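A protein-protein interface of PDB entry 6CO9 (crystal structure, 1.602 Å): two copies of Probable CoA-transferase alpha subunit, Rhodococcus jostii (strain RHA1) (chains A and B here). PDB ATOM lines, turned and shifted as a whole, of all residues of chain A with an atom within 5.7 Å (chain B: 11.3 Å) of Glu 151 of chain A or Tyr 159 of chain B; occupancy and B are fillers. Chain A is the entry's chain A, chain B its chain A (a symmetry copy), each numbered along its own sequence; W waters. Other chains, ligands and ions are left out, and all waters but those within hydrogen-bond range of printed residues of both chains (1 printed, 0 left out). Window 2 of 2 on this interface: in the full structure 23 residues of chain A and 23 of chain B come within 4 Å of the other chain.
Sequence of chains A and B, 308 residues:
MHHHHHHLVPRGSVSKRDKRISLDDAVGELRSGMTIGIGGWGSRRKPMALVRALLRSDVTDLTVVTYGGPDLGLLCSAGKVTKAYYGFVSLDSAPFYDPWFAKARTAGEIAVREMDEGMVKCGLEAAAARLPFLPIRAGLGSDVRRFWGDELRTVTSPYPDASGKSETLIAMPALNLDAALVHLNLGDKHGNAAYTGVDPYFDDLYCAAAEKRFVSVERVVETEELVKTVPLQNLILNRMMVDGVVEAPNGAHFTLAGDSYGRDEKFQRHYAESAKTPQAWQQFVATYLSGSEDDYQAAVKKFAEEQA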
ATOM      1  N   LYS A  83      10.870  20.168  45.878  1.00  0.00           N
ATOM      2  CA  LYS A  83      10.324  19.968  44.547  1.00  0.00           C
ATOM      3  C   LYS A  83       9.653  18.607  44.539  1.00  0.00           C
ATOM      4  O   LYS A  83      10.171  17.656  45.129  1.00  0.00           O
ATOM      5  CB  LYS A  83      11.429  20.060  43.486  1.00  0.00           C
ATOM      6  CG  LYS A  83      10.949  20.020  42.033  1.00  0.00           C
ATOM      7  CD  LYS A  83      12.085  20.415  41.080  1.00  0.00           C
ATOM      8  CE  LYS A  83      11.617  20.433  39.620  1.00  0.00           C
ATOM      9  NZ  LYS A  83      12.725  20.607  38.613  1.00  0.00           N
ATOM     10  N   TYR A  85       7.568  15.693  42.072  1.00  0.00           N
ATOM     11  CA  TYR A  85       7.102  15.085  40.833  1.00  0.00           C
ATOM     12  C   TYR A  85       6.054  14.041  41.200  1.00  0.00           C
ATOM     13  O   TYR A  85       6.370  13.080  41.903  1.00  0.00           O
ATOM     14  CB  TYR A  85       8.257  14.403  40.104  1.00  0.00           C
ATOM     15  CG  TYR A  85       9.333  15.302  39.543  1.00  0.00           C
ATOM     16  CD1 TYR A  85      10.296  15.865  40.373  1.00  0.00           C
ATOM     17  CD2 TYR A  85       9.394  15.574  38.180  1.00  0.00           C
ATOM     18  CE1 TYR A  85      11.294  16.681  39.858  1.00  0.00           C
ATOM     19  CE2 TYR A  85      10.392  16.384  37.650  1.00  0.00           C
ATOM     20  CZ  TYR A  85      11.338  16.933  38.496  1.00  0.00           C
ATOM     21  OH  TYR A  85      12.338  17.741  38.000  1.00  0.00           O
ATOM     22  N   ARG A 113       6.236  19.521  39.674  1.00  0.00           N
ATOM     23  CA  ARG A 113       6.168  19.007  38.314  1.00  0.00           C
ATOM     24  C   ARG A 113       5.080  17.946  38.289  1.00  0.00           C
ATOM     25  O   ARG A 113       5.339  16.750  38.121  1.00  0.00           O
ATOM     26  CB  ARG A 113       7.522  18.467  37.861  1.00  0.00           C
ATOM     27  CG  ARG A 113       8.610  19.537  37.819  1.00  0.00           C
ATOM     28  CD  ARG A 113       8.309  20.618  36.780  1.00  0.00           C
ATOM     29  NE  ARG A 113       9.362  21.631  36.767  1.00  0.00           N
ATOM     30  CZ  ARG A 113       9.340  22.736  37.505  1.00  0.00           C
ATOM     31  NH1 ARG A 113       8.305  22.973  38.302  1.00  0.00           N
ATOM     32  NH2 ARG A 113      10.347  23.605  37.446  1.00  0.00           N
ATOM     33  N   PRO A 132      17.122   8.448  27.878  1.00  0.00           N
ATOM     34  CA  PRO A 132      16.862   9.851  28.264  1.00  0.00           C
ATOM     35  C   PRO A 132      15.395  10.231  28.223  1.00  0.00           C
ATOM     36  O   PRO A 132      15.006  11.209  28.884  1.00  0.00           O
ATOM     37  CB  PRO A 132      17.672  10.657  27.238  1.00  0.00           C
ATOM     38  CG  PRO A 132      17.733   9.746  26.024  1.00  0.00           C
ATOM     39  CD  PRO A 132      17.792   8.340  26.568  1.00  0.00           C
ATOM     40  N   PHE A 133      14.567   9.506  27.474  1.00  0.00           N
ATOM     41  CA  PHE A 133      13.146   9.809  27.398  1.00  0.00           C
ATOM     42  C   PHE A 133      12.414   8.579  26.893  1.00  0.00           C
ATOM     43  O   PHE A 133      13.021   7.673  26.317  1.00  0.00           O
ATOM     44  CB  PHE A 133      12.869  10.978  26.442  1.00  0.00           C
ATOM     45  CG  PHE A 133      12.969  10.583  24.979  1.00  0.00           C
ATOM     46  CD1 PHE A 133      14.199  10.555  24.335  1.00  0.00           C
ATOM     47  CD2 PHE A 133      11.837  10.213  24.261  1.00  0.00           C
ATOM     48  CE1 PHE A 133      14.304  10.173  23.007  1.00  0.00           C
ATOM     49  CE2 PHE A 133      11.938   9.812  22.920  1.00  0.00           C
ATOM     50  CZ  PHE A 133      13.176   9.808  22.297  1.00  0.00           C
ATOM     51  N   TRP A 148       5.434  22.136  33.755  1.00  0.00           N
ATOM     52  CA  TRP A 148       6.828  21.816  33.463  1.00  0.00           C
ATOM     53  C   TRP A 148       7.559  22.877  32.654  1.00  0.00           C
ATOM     54  O   TRP A 148       8.791  22.965  32.749  1.00  0.00           O
ATOM     55  CB  TRP A 148       6.915  20.503  32.691  1.00  0.00           C
ATOM     56  CG  TRP A 148       6.597  19.283  33.467  1.00  0.00           C
ATOM     57  CD1 TRP A 148       5.394  18.946  34.027  1.00  0.00           C
ATOM     58  CD2 TRP A 148       7.487  18.190  33.725  1.00  0.00           C
ATOM     59  NE1 TRP A 148       5.492  17.713  34.640  1.00  0.00           N
ATOM     60  CE2 TRP A 148       6.762  17.226  34.461  1.00  0.00           C
ATOM     61  CE3 TRP A 148       8.833  17.937  33.417  1.00  0.00           C
ATOM     62  CZ2 TRP A 148       7.338  16.031  34.898  1.00  0.00           C
ATOM     63  CZ3 TRP A 148       9.405  16.746  33.847  1.00  0.00           C
ATOM     64  CH2 TRP A 148       8.654  15.804  34.575  1.00  0.00           C
ATOM     65  N   GLY A 149       6.853  23.650  31.828  1.00  0.00           N
ATOM     66  CA  GLY A 149       7.549  24.580  30.951  1.00  0.00           C
ATOM     67  C   GLY A 149       8.543  23.855  30.064  1.00  0.00           C
ATOM     68  O   GLY A 149       8.260  22.777  29.533  1.00  0.00           O
ATOM     69  N   ASP A 150       9.739  24.436  29.919  1.00  0.00           N
ATOM     70  CA  ASP A 150      10.717  23.872  28.993  1.00  0.00           C
ATOM     71  C   ASP A 150      11.397  22.617  29.527  1.00  0.00           C
ATOM     72  O   ASP A 150      12.182  22.002  28.795  1.00  0.00           O
ATOM     73  CB  ASP A 150      11.771  24.923  28.619  1.00  0.00           C
ATOM     74  CG  ASP A 150      12.623  24.493  27.439  1.00  0.00           C
ATOM     75  OD1 ASP A 150      12.043  24.047  26.416  1.00  0.00           O
ATOM     76  OD2 ASP A 150      13.865  24.602  27.533  1.00  0.00           O
ATOM     77  N   GLU A 151      11.114  22.207  30.769  1.00  0.00           N
ATOM     78  CA  GLU A 151      11.614  20.925  31.249  1.00  0.00           C
ATOM     79  C   GLU A 151      10.910  19.753  30.571  1.00  0.00           C
ATOM     80  O   GLU A 151      11.427  18.633  30.598  1.00  0.00           O
ATOM     81  CB  GLU A 151      11.466  20.845  32.778  1.00  0.00           C
ATOM     82  CG  GLU A 151      12.110  19.605  33.410  1.00  0.00           C
ATOM     83  CD  GLU A 151      12.015  19.540  34.931  1.00  0.00           C
ATOM     84  OE1 GLU A 151      12.262  18.437  35.471  1.00  0.00           O
ATOM     85  OE2 GLU A 151      11.724  20.577  35.584  1.00  0.00           O
ATOM     86  N   LEU A 152       9.754  19.985  29.951  1.00  0.00           N
ATOM     87  CA  LEU A 152       9.017  18.937  29.245  1.00  0.00           C
ATOM     88  C   LEU A 152       8.922  19.331  27.777  1.00  0.00           C
ATOM     89  O   LEU A 152       8.268  20.322  27.434  1.00  0.00           O
ATOM     90  CB  LEU A 152       7.629  18.732  29.851  1.00  0.00           C
ATOM     91  CG  LEU A 152       6.832  17.531  29.352  1.00  0.00           C
ATOM     92  CD1 LEU A 152       7.542  16.226  29.732  1.00  0.00           C
ATOM     93  CD2 LEU A 152       5.428  17.580  29.928  1.00  0.00           C
ATOM     94  N   ARG A 153       9.586  18.564  26.917  1.00  0.00           N
ATOM     95  CA  ARG A 153       9.625  18.826  25.487  1.00  0.00           C
ATOM     96  C   ARG A 153       8.899  17.719  24.742  1.00  0.00           C
ATOM     97  O   ARG A 153       8.595  16.664  25.300  1.00  0.00           O
ATOM     98  CB  ARG A 153      11.073  18.936  24.994  1.00  0.00           C
ATOM     99  CG  ARG A 153      11.774  20.142  25.609  1.00  0.00           C
ATOM    100  CD  ARG A 153      13.280  20.118  25.441  1.00  0.00           C
ATOM    101  NE  ARG A 153      13.874  21.345  25.982  1.00  0.00           N
ATOM    102  CZ  ARG A 153      15.180  21.590  26.047  1.00  0.00           C
ATOM    103  NH1 ARG A 153      16.058  20.692  25.616  1.00  0.00           N
ATOM    104  NH2 ARG A 153      15.612  22.740  26.548  1.00  0.00           N
ATOM    105  N   THR A 154       8.629  17.986  23.467  1.00  0.00           N
ATOM    106  CA  THR A 154       8.030  16.989  22.593  1.00  0.00           C
ATOM    107  C   THR A 154       9.095  16.315  21.746  1.00  0.00           C
ATOM    108  O   THR A 154      10.238  16.774  21.640  1.00  0.00           O
ATOM    109  CB  THR A 154       6.969  17.610  21.686  1.00  0.00           C
ATOM    110  OG1 THR A 154       7.568  18.624  20.869  1.00  0.00           O
ATOM    111  CG2 THR A 154       5.842  18.214  22.516  1.00  0.00           C
ATOM    112  N   ALA A 171       7.828  13.911  25.076  1.00  0.00           N
ATOM    113  CA  ALA A 171       9.058  13.190  25.397  1.00  0.00           C
ATOM    114  C   ALA A 171       9.177  13.188  26.909  1.00  0.00           C
ATOM    115  O   ALA A 171       9.665  14.149  27.508  1.00  0.00           O
ATOM    116  CB  ALA A 171      10.269  13.849  24.752  1.00  0.00           C
ATOM    117  N   MET A 172       8.699  12.130  27.545  1.00  0.00           N
ATOM    118  CA  MET A 172       8.772  12.066  29.002  1.00  0.00           C
ATOM    119  C   MET A 172      10.215  11.832  29.423  1.00  0.00           C
ATOM    120  O   MET A 172      10.788  10.791  29.079  1.00  0.00           O
ATOM    121  CB  MET A 172       7.880  10.952  29.534  1.00  0.00           C
ATOM    122  CG  MET A 172       7.970  10.804  31.040  1.00  0.00           C
ATOM    123  SD  MET A 172       7.356  12.261  31.893  1.00  0.00           S
ATOM    124  CE  MET A 172       8.146  12.006  33.483  1.00  0.00           C
ATOM    125  N   PRO A 173      10.844  12.752  30.153  1.00  0.00           N
ATOM    126  CA  PRO A 173      12.244  12.537  30.528  1.00  0.00           C
ATOM    127  C   PRO A 173      12.358  11.460  31.598  1.00  0.00           C
ATOM    128  O   PRO A 173      11.438  11.231  32.386  1.00  0.00           O
ATOM    129  CB  PRO A 173      12.688  13.902  31.071  1.00  0.00           C
ATOM    130  CG  PRO A 173      11.398  14.514  31.616  1.00  0.00           C
ATOM    131  CD  PRO A 173      10.314  14.034  30.655  1.00  0.00           C
ATOM    132  N   PHE B 133       6.620   4.659  17.388  1.00  0.00           N
ATOM    133  CA  PHE B 133       7.950   4.127  17.646  1.00  0.00           C
ATOM    134  C   PHE B 133       8.181   4.108  19.146  1.00  0.00           C
ATOM    135  O   PHE B 133       7.483   4.786  19.904  1.00  0.00           O
ATOM    136  CB  PHE B 133       9.039   4.986  16.988  1.00  0.00           C
ATOM    137  CG  PHE B 133       9.300   6.284  17.733  1.00  0.00           C
ATOM    138  CD1 PHE B 133       8.506   7.401  17.509  1.00  0.00           C
ATOM    139  CD2 PHE B 133      10.320   6.373  18.673  1.00  0.00           C
ATOM    140  CE1 PHE B 133       8.721   8.582  18.200  1.00  0.00           C
ATOM    141  CE2 PHE B 133      10.534   7.562  19.387  1.00  0.00           C
ATOM    142  CZ  PHE B 133       9.738   8.667  19.134  1.00  0.00           C
ATOM    143  N   PRO B 135      12.036   4.348  21.473  1.00  0.00           N
ATOM    144  CA  PRO B 135      13.495   4.389  21.352  1.00  0.00           C
ATOM    145  C   PRO B 135      14.131   3.203  22.052  1.00  0.00           C
ATOM    146  O   PRO B 135      13.634   2.708  23.069  1.00  0.00           O
ATOM    147  CB  PRO B 135      13.865   5.695  22.061  1.00  0.00           C
ATOM    148  CG  PRO B 135      12.804   5.801  23.140  1.00  0.00           C
ATOM    149  CD  PRO B 135      11.537   5.301  22.482  1.00  0.00           C
ATOM    150  N   VAL B 155      16.272   8.341  16.275  1.00  0.00           N
ATOM    151  CA  VAL B 155      15.592   9.464  16.905  1.00  0.00           C
ATOM    152  C   VAL B 155      16.541  10.061  17.936  1.00  0.00           C
ATOM    153  O   VAL B 155      17.178   9.329  18.704  1.00  0.00           O
ATOM    154  CB  VAL B 155      14.257   9.040  17.552  1.00  0.00           C
ATOM    155  CG1 VAL B 155      14.476   7.930  18.597  1.00  0.00           C
ATOM    156  CG2 VAL B 155      13.588  10.248  18.209  1.00  0.00           C
ATOM    157  N   THR B 156      16.642  11.385  17.949  1.00  0.00           N
ATOM    158  CA  THR B 156      17.525  12.089  18.875  1.00  0.00           C
ATOM    159  C   THR B 156      16.737  12.601  20.070  1.00  0.00           C
ATOM    160  O   THR B 156      15.637  13.142  19.915  1.00  0.00           O
ATOM    161  CB  THR B 156      18.235  13.239  18.168  1.00  0.00           C
ATOM    162  OG1 THR B 156      19.002  12.709  17.079  1.00  0.00           O
ATOM    163  CG2 THR B 156      19.183  13.955  19.121  1.00  0.00           C
ATOM    164  N   SER B 157      17.296  12.410  21.255  1.00  0.00           N
ATOM    165  CA  SER B 157      16.666  12.904  22.472  1.00  0.00           C
ATOM    166  C   SER B 157      16.537  14.423  22.426  1.00  0.00           C
ATOM    167  O   SER B 157      17.512  15.115  22.094  1.00  0.00           O
ATOM    168  CB  SER B 157      17.492  12.498  23.688  1.00  0.00           C
ATOM    169  OG  SER B 157      16.971  13.091  24.861  1.00  0.00           O
ATOM    170  N   PRO B 158      15.377  14.985  22.781  1.00  0.00           N
ATOM    171  CA  PRO B 158      15.293  16.442  22.940  1.00  0.00           C
ATOM    172  C   PRO B 158      15.978  16.929  24.197  1.00  0.00           C
ATOM    173  O   PRO B 158      16.105  18.149  24.381  1.00  0.00           O
ATOM    174  CB  PRO B 158      13.783  16.708  22.984  1.00  0.00           C
ATOM    175  CG  PRO B 158      13.190  15.435  23.471  1.00  0.00           C
ATOM    176  CD  PRO B 158      14.069  14.325  22.967  1.00  0.00           C
ATOM    177  N   TYR B 159      16.434  16.020  25.058  1.00  0.00           N
ATOM    178  CA  TYR B 159      17.140  16.383  26.281  1.00  0.00           C
ATOM    179  C   TYR B 159      18.583  15.931  26.150  1.00  0.00           C
ATOM    180  O   TYR B 159      18.839  14.720  26.085  1.00  0.00           O
ATOM    181  CB  TYR B 159      16.496  15.726  27.506  1.00  0.00           C
ATOM    182  CG  TYR B 159      15.007  15.890  27.572  1.00  0.00           C
ATOM    183  CD1 TYR B 159      14.438  17.118  27.896  1.00  0.00           C
ATOM    184  CD2 TYR B 159      14.165  14.819  27.333  1.00  0.00           C
ATOM    185  CE1 TYR B 159      13.072  17.274  27.962  1.00  0.00           C
ATOM    186  CE2 TYR B 159      12.800  14.961  27.391  1.00  0.00           C
ATOM    187  CZ  TYR B 159      12.252  16.189  27.710  1.00  0.00           C
ATOM    188  OH  TYR B 159      10.893  16.319  27.764  1.00  0.00           O
ATOM    189  N   PRO B 160      19.554  16.837  26.086  1.00  0.00           N
ATOM    190  CA  PRO B 160      20.951  16.399  26.123  1.00  0.00           C
ATOM    191  C   PRO B 160      21.261  15.737  27.455  1.00  0.00           C
ATOM    192  O   PRO B 160      20.604  15.997  28.472  1.00  0.00           O
ATOM    193  CB  PRO B 160      21.739  17.707  25.955  1.00  0.00           C
ATOM    194  CG  PRO B 160      20.738  18.678  25.345  1.00  0.00           C
ATOM    195  CD  PRO B 160      19.432  18.298  25.970  1.00  0.00           C
ATOM    196  N   ASP B 161      22.272  14.875  27.454  1.00  0.00           N
ATOM    197  CA  ASP B 161      22.772  14.337  28.705  1.00  0.00           C
ATOM    198  C   ASP B 161      23.477  15.448  29.490  1.00  0.00           C
ATOM    199  O   ASP B 161      23.668  16.571  29.002  1.00  0.00           O
ATOM    200  CB  ASP B 161      23.711  13.152  28.448  1.00  0.00           C
ATOM    201  CG  ASP B 161      22.986  11.905  27.899  1.00  0.00           C
ATOM    202  OD1 ASP B 161      21.755  11.936  27.672  1.00  0.00           O
ATOM    203  OD2 ASP B 161      23.661  10.870  27.703  1.00  0.00           O
ATOM    204  N   ALA B 162      23.882  15.123  30.720  1.00  0.00           N
ATOM    205  CA  ALA B 162      24.518  16.115  31.584  1.00  0.00           C
ATOM    206  C   ALA B 162      25.704  16.793  30.901  1.00  0.00           C
ATOM    207  O   ALA B 162      25.880  18.013  31.013  1.00  0.00           O
ATOM    208  CB  ALA B 162      24.956  15.451  32.890  1.00  0.00           C
ATOM    209  N   SER B 163      26.508  16.023  30.156  1.00  0.00           N
ATOM    210  CA  SER B 163      27.700  16.551  29.497  1.00  0.00           C
ATOM    211  C   SER B 163      27.381  17.534  28.379  1.00  0.00           C
ATOM    212  O   SER B 163      28.294  18.213  27.890  1.00  0.00           O
ATOM    213  CB  SER B 163      28.529  15.407  28.922  1.00  0.00           C
ATOM    214  OG  SER B 163      27.849  14.809  27.830  1.00  0.00           O
ATOM    215  N   GLY B 164      26.126  17.623  27.959  1.00  0.00           N
ATOM    216  CA  GLY B 164      25.749  18.471  26.858  1.00  0.00           C
ATOM    217  C   GLY B 164      25.556  17.737  25.548  1.00  0.00           C
ATOM    218  O   GLY B 164      25.134  18.363  24.573  1.00  0.00           O
ATOM    219  N   LYS B 165      25.841  16.438  25.499  1.00  0.00           N
ATOM    220  CA  LYS B 165      25.671  15.639  24.288  1.00  0.00           C
ATOM    221  C   LYS B 165      24.301  14.977  24.272  1.00  0.00           C
ATOM    222  O   LYS B 165      23.864  14.414  25.278  1.00  0.00           O
ATOM    223  CB  LYS B 165      26.732  14.542  24.187  1.00  0.00           C
ATOM    224  CG  LYS B 165      28.164  15.003  24.109  1.00  0.00           C
ATOM    225  CD  LYS B 165      29.083  13.788  24.048  1.00  0.00           C
ATOM    226  CE  LYS B 165      30.512  14.180  23.752  1.00  0.00           C
ATOM    227  NZ  LYS B 165      31.146  14.763  24.960  1.00  0.00           N
ATOM    228  N   SER B 166      23.641  15.019  23.118  1.00  0.00           N
ATOM    229  CA  SER B 166      22.336  14.387  22.953  1.00  0.00           C
ATOM    230  C   SER B 166      22.479  12.979  22.397  1.00  0.00           C
ATOM    231  O   SER B 166      23.246  12.747  21.452  1.00  0.00           O
ATOM    232  CB  SER B 166      21.442  15.222  22.042  1.00  0.00           C
ATOM    233  OG  SER B 166      21.398  16.567  22.500  1.00  0.00           O
ATOM    234  N   GLU B 167      21.735  12.052  22.986  1.00  0.00           N
ATOM    235  CA  GLU B 167      21.757  10.669  22.533  1.00  0.00           C
ATOM    236  C   GLU B 167      20.887  10.496  21.301  1.00  0.00           C
ATOM    237  O   GLU B 167      19.768  11.021  21.235  1.00  0.00           O
ATOM    238  CB  GLU B 167      21.254   9.736  23.629  1.00  0.00           C
ATOM    239  CG  GLU B 167      22.159   9.620  24.816  1.00  0.00           C
ATOM    240  CD  GLU B 167      21.725   8.506  25.742  1.00  0.00           C
ATOM    241  OE1 GLU B 167      20.999   7.606  25.277  1.00  0.00           O
ATOM    242  OE2 GLU B 167      22.089   8.539  26.933  1.00  0.00           O
ATOM    243  N   THR B 168      21.396   9.729  20.338  1.00  0.00           N
ATOM    244  CA  THR B 168      20.651   9.322  19.158  1.00  0.00           C
ATOM    245  C   THR B 168      20.461   7.817  19.261  1.00  0.00           C
ATOM    246  O   THR B 168      21.438   7.073  19.396  1.00  0.00           O
ATOM    247  CB  THR B 168      21.389   9.706  17.876  1.00  0.00           C
ATOM    248  OG1 THR B 168      21.441  11.135  17.766  1.00  0.00           O
ATOM    249  CG2 THR B 168      20.670   9.150  16.663  1.00  0.00           C
ATOM    250  N   LEU B 169      19.209   7.384  19.255  1.00  0.00           N
ATOM    251  CA  LEU B 169      18.842   6.004  19.514  1.00  0.00           C
ATOM    252  C   LEU B 169      18.127   5.427  18.307  1.00  0.00           C
ATOM    253  O   LEU B 169      17.679   6.159  17.423  1.00  0.00           O
ATOM    254  CB  LEU B 169      17.927   5.905  20.732  1.00  0.00           C
ATOM    255  CG  LEU B 169      18.579   6.410  22.006  1.00  0.00           C
ATOM    256  CD1 LEU B 169      17.536   6.973  22.969  1.00  0.00           C
ATOM    257  CD2 LEU B 169      19.344   5.271  22.610  1.00  0.00           C
HETATM  258  O   HOH W   1      15.457  19.851  22.311  1.00  0.00           O
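Position printed for both chains: 133. Of the 13 pairs that touch across the chains among the printed residues, none has its exchanged pair printed and touching as well.
The side-chain amino group of Lys 83 of chain A lies within salt-bridge range of the side-chain carboxylate of Glu 151 of chain A (3.2 Å). OE2 of Glu 151 of chain A is in salt-bridge range of NE of Arg 113 of chain A, 2.8 Å away. OD2 of Asp 150 of chain A is in salt-bridge range of NH2 of Arg 153 of chain A (2.7 Å). N of Val 155 of chain B sits at hydrogen-bond distance from O of Leu 169 of chain B (2.8 Å). The side-chain hydroxyl of Ser 157 of chain B is in hydrogen-bond range of the backbone carbonyl oxygen of Tyr 159 of chain B (2.8 Å). The backbone NH (N) of Ser 157 of chain B sits at hydrogen-bond distance from the backbone carbonyl oxygen (O) of Glu 167 of chain B, 2.8 Å away.
Arg 113 of chain A touches none of the printed residues of chain B. Of the printed residues of chain B, Pro 132 of chain A touches Ser 157 (3.5 Å), Glu 167 (3.5 Å) and Leu 169 (3.9 Å). No residue of chain B comes within 4 Å of Trp 148 of chain A. No residue of chain B comes within 4 Å of Gly 149 of chain A. No residue of chain B comes within 4 Å of Asp 150 of chain A. Printed residues of chain B within 4 Å of Glu 151 of chain A: Tyr 159. Arg 153 of chain A touches two residues of chain B. Met 172 of chain A touches none of the printed residues of chain B. Printed residues of chain B within 4 Å of Pro 173 of chain A: Tyr 159. Printed residues of chain A within 4 Å of Pro 135 of chain B: Phe 133 (3.7 Å). Printed residues of chain A within 4 Å of Ser 157 of chain B: Pro 132 and Phe 133. Of the printed residues of chain A, Pro 158 of chain B touches Arg 153, Thr 154 and Ala 171. Of the printed residues of chain A, Tyr 159 of chain B touches Glu 151 (3.4 Å), Leu 152 (3.5 Å), Arg 153 (2.7 Å), Ala 171 (2.5 Å) and Pro 173 (3.7 Å). Of the printed residues of chain A, Glu 167 of chain B touches Pro 132. The nearest printed residue of chain A that does not touch Tyr 159 of chain B is Pro 132 of chain A (4.02 Å).
Among the printed residues, pairs that only touch across the chains: Pro 132 of chain A with Ser 157 of chain B (3.5 Å), Pro 132 of chain A with Glu 167 of chain B (3.5 Å), Pro 132 of chain A with Leu 169 of chain B (3.9 Å), Phe 133 of chain A with Pro 135 of chain B (3.7 Å), Phe 133 of chain A with Ser 157 of chain B (3.7 Å), Glu 151 of chain A with Tyr 159 of chain B (3.4 Å), Leu 152 of chain A with Tyr 159 of chain B (3.5 Å), Thr 154 of chain A with Pro 158 of chain B (3.7 Å), Ala 171 of chain A with Pro 158 of chain B (3.6 Å) and Pro 173 of chain A with Tyr 159 of chain B (3.7 Å).
Water W1 lies within hydrogen-bond range of O of Pro 158 of chain B and NH1 of Arg 153 of chain A.
Of the 17 printed residues of chain B, 6 touch a printed residue of chain A. Of the 15 printed residues of chain A, 8 touch a printed residue of chain B. Printed residues of chain A that touch a printed residue of chain B: Pro 132, Phe 133, Glu 151, Leu 152, Arg 153, Thr 154, Ala 171 and Pro 173. Hydrophobic or aromatic side chains of chain A that line the printed part of chain B: Pro 132, Phe 133, Leu 152, Ala 171 and Pro 173. Along chain A the printed residues that touch a printed residue of chain B span positions 132 to 173.
NH1 of Arg 153 of chain A is in hydrogen-bond range of O of Pro 158 of chain B, at 2.8 Å. The backbone NH (N) of Arg 153 of chain A sits at hydrogen-bond distance from the side-chain hydroxyl (OH) of Tyr 159 of chain B. O of Ala 171 of chain A sits at hydrogen-bond distance from OH of Tyr 159 of chain B (2.5 Å).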
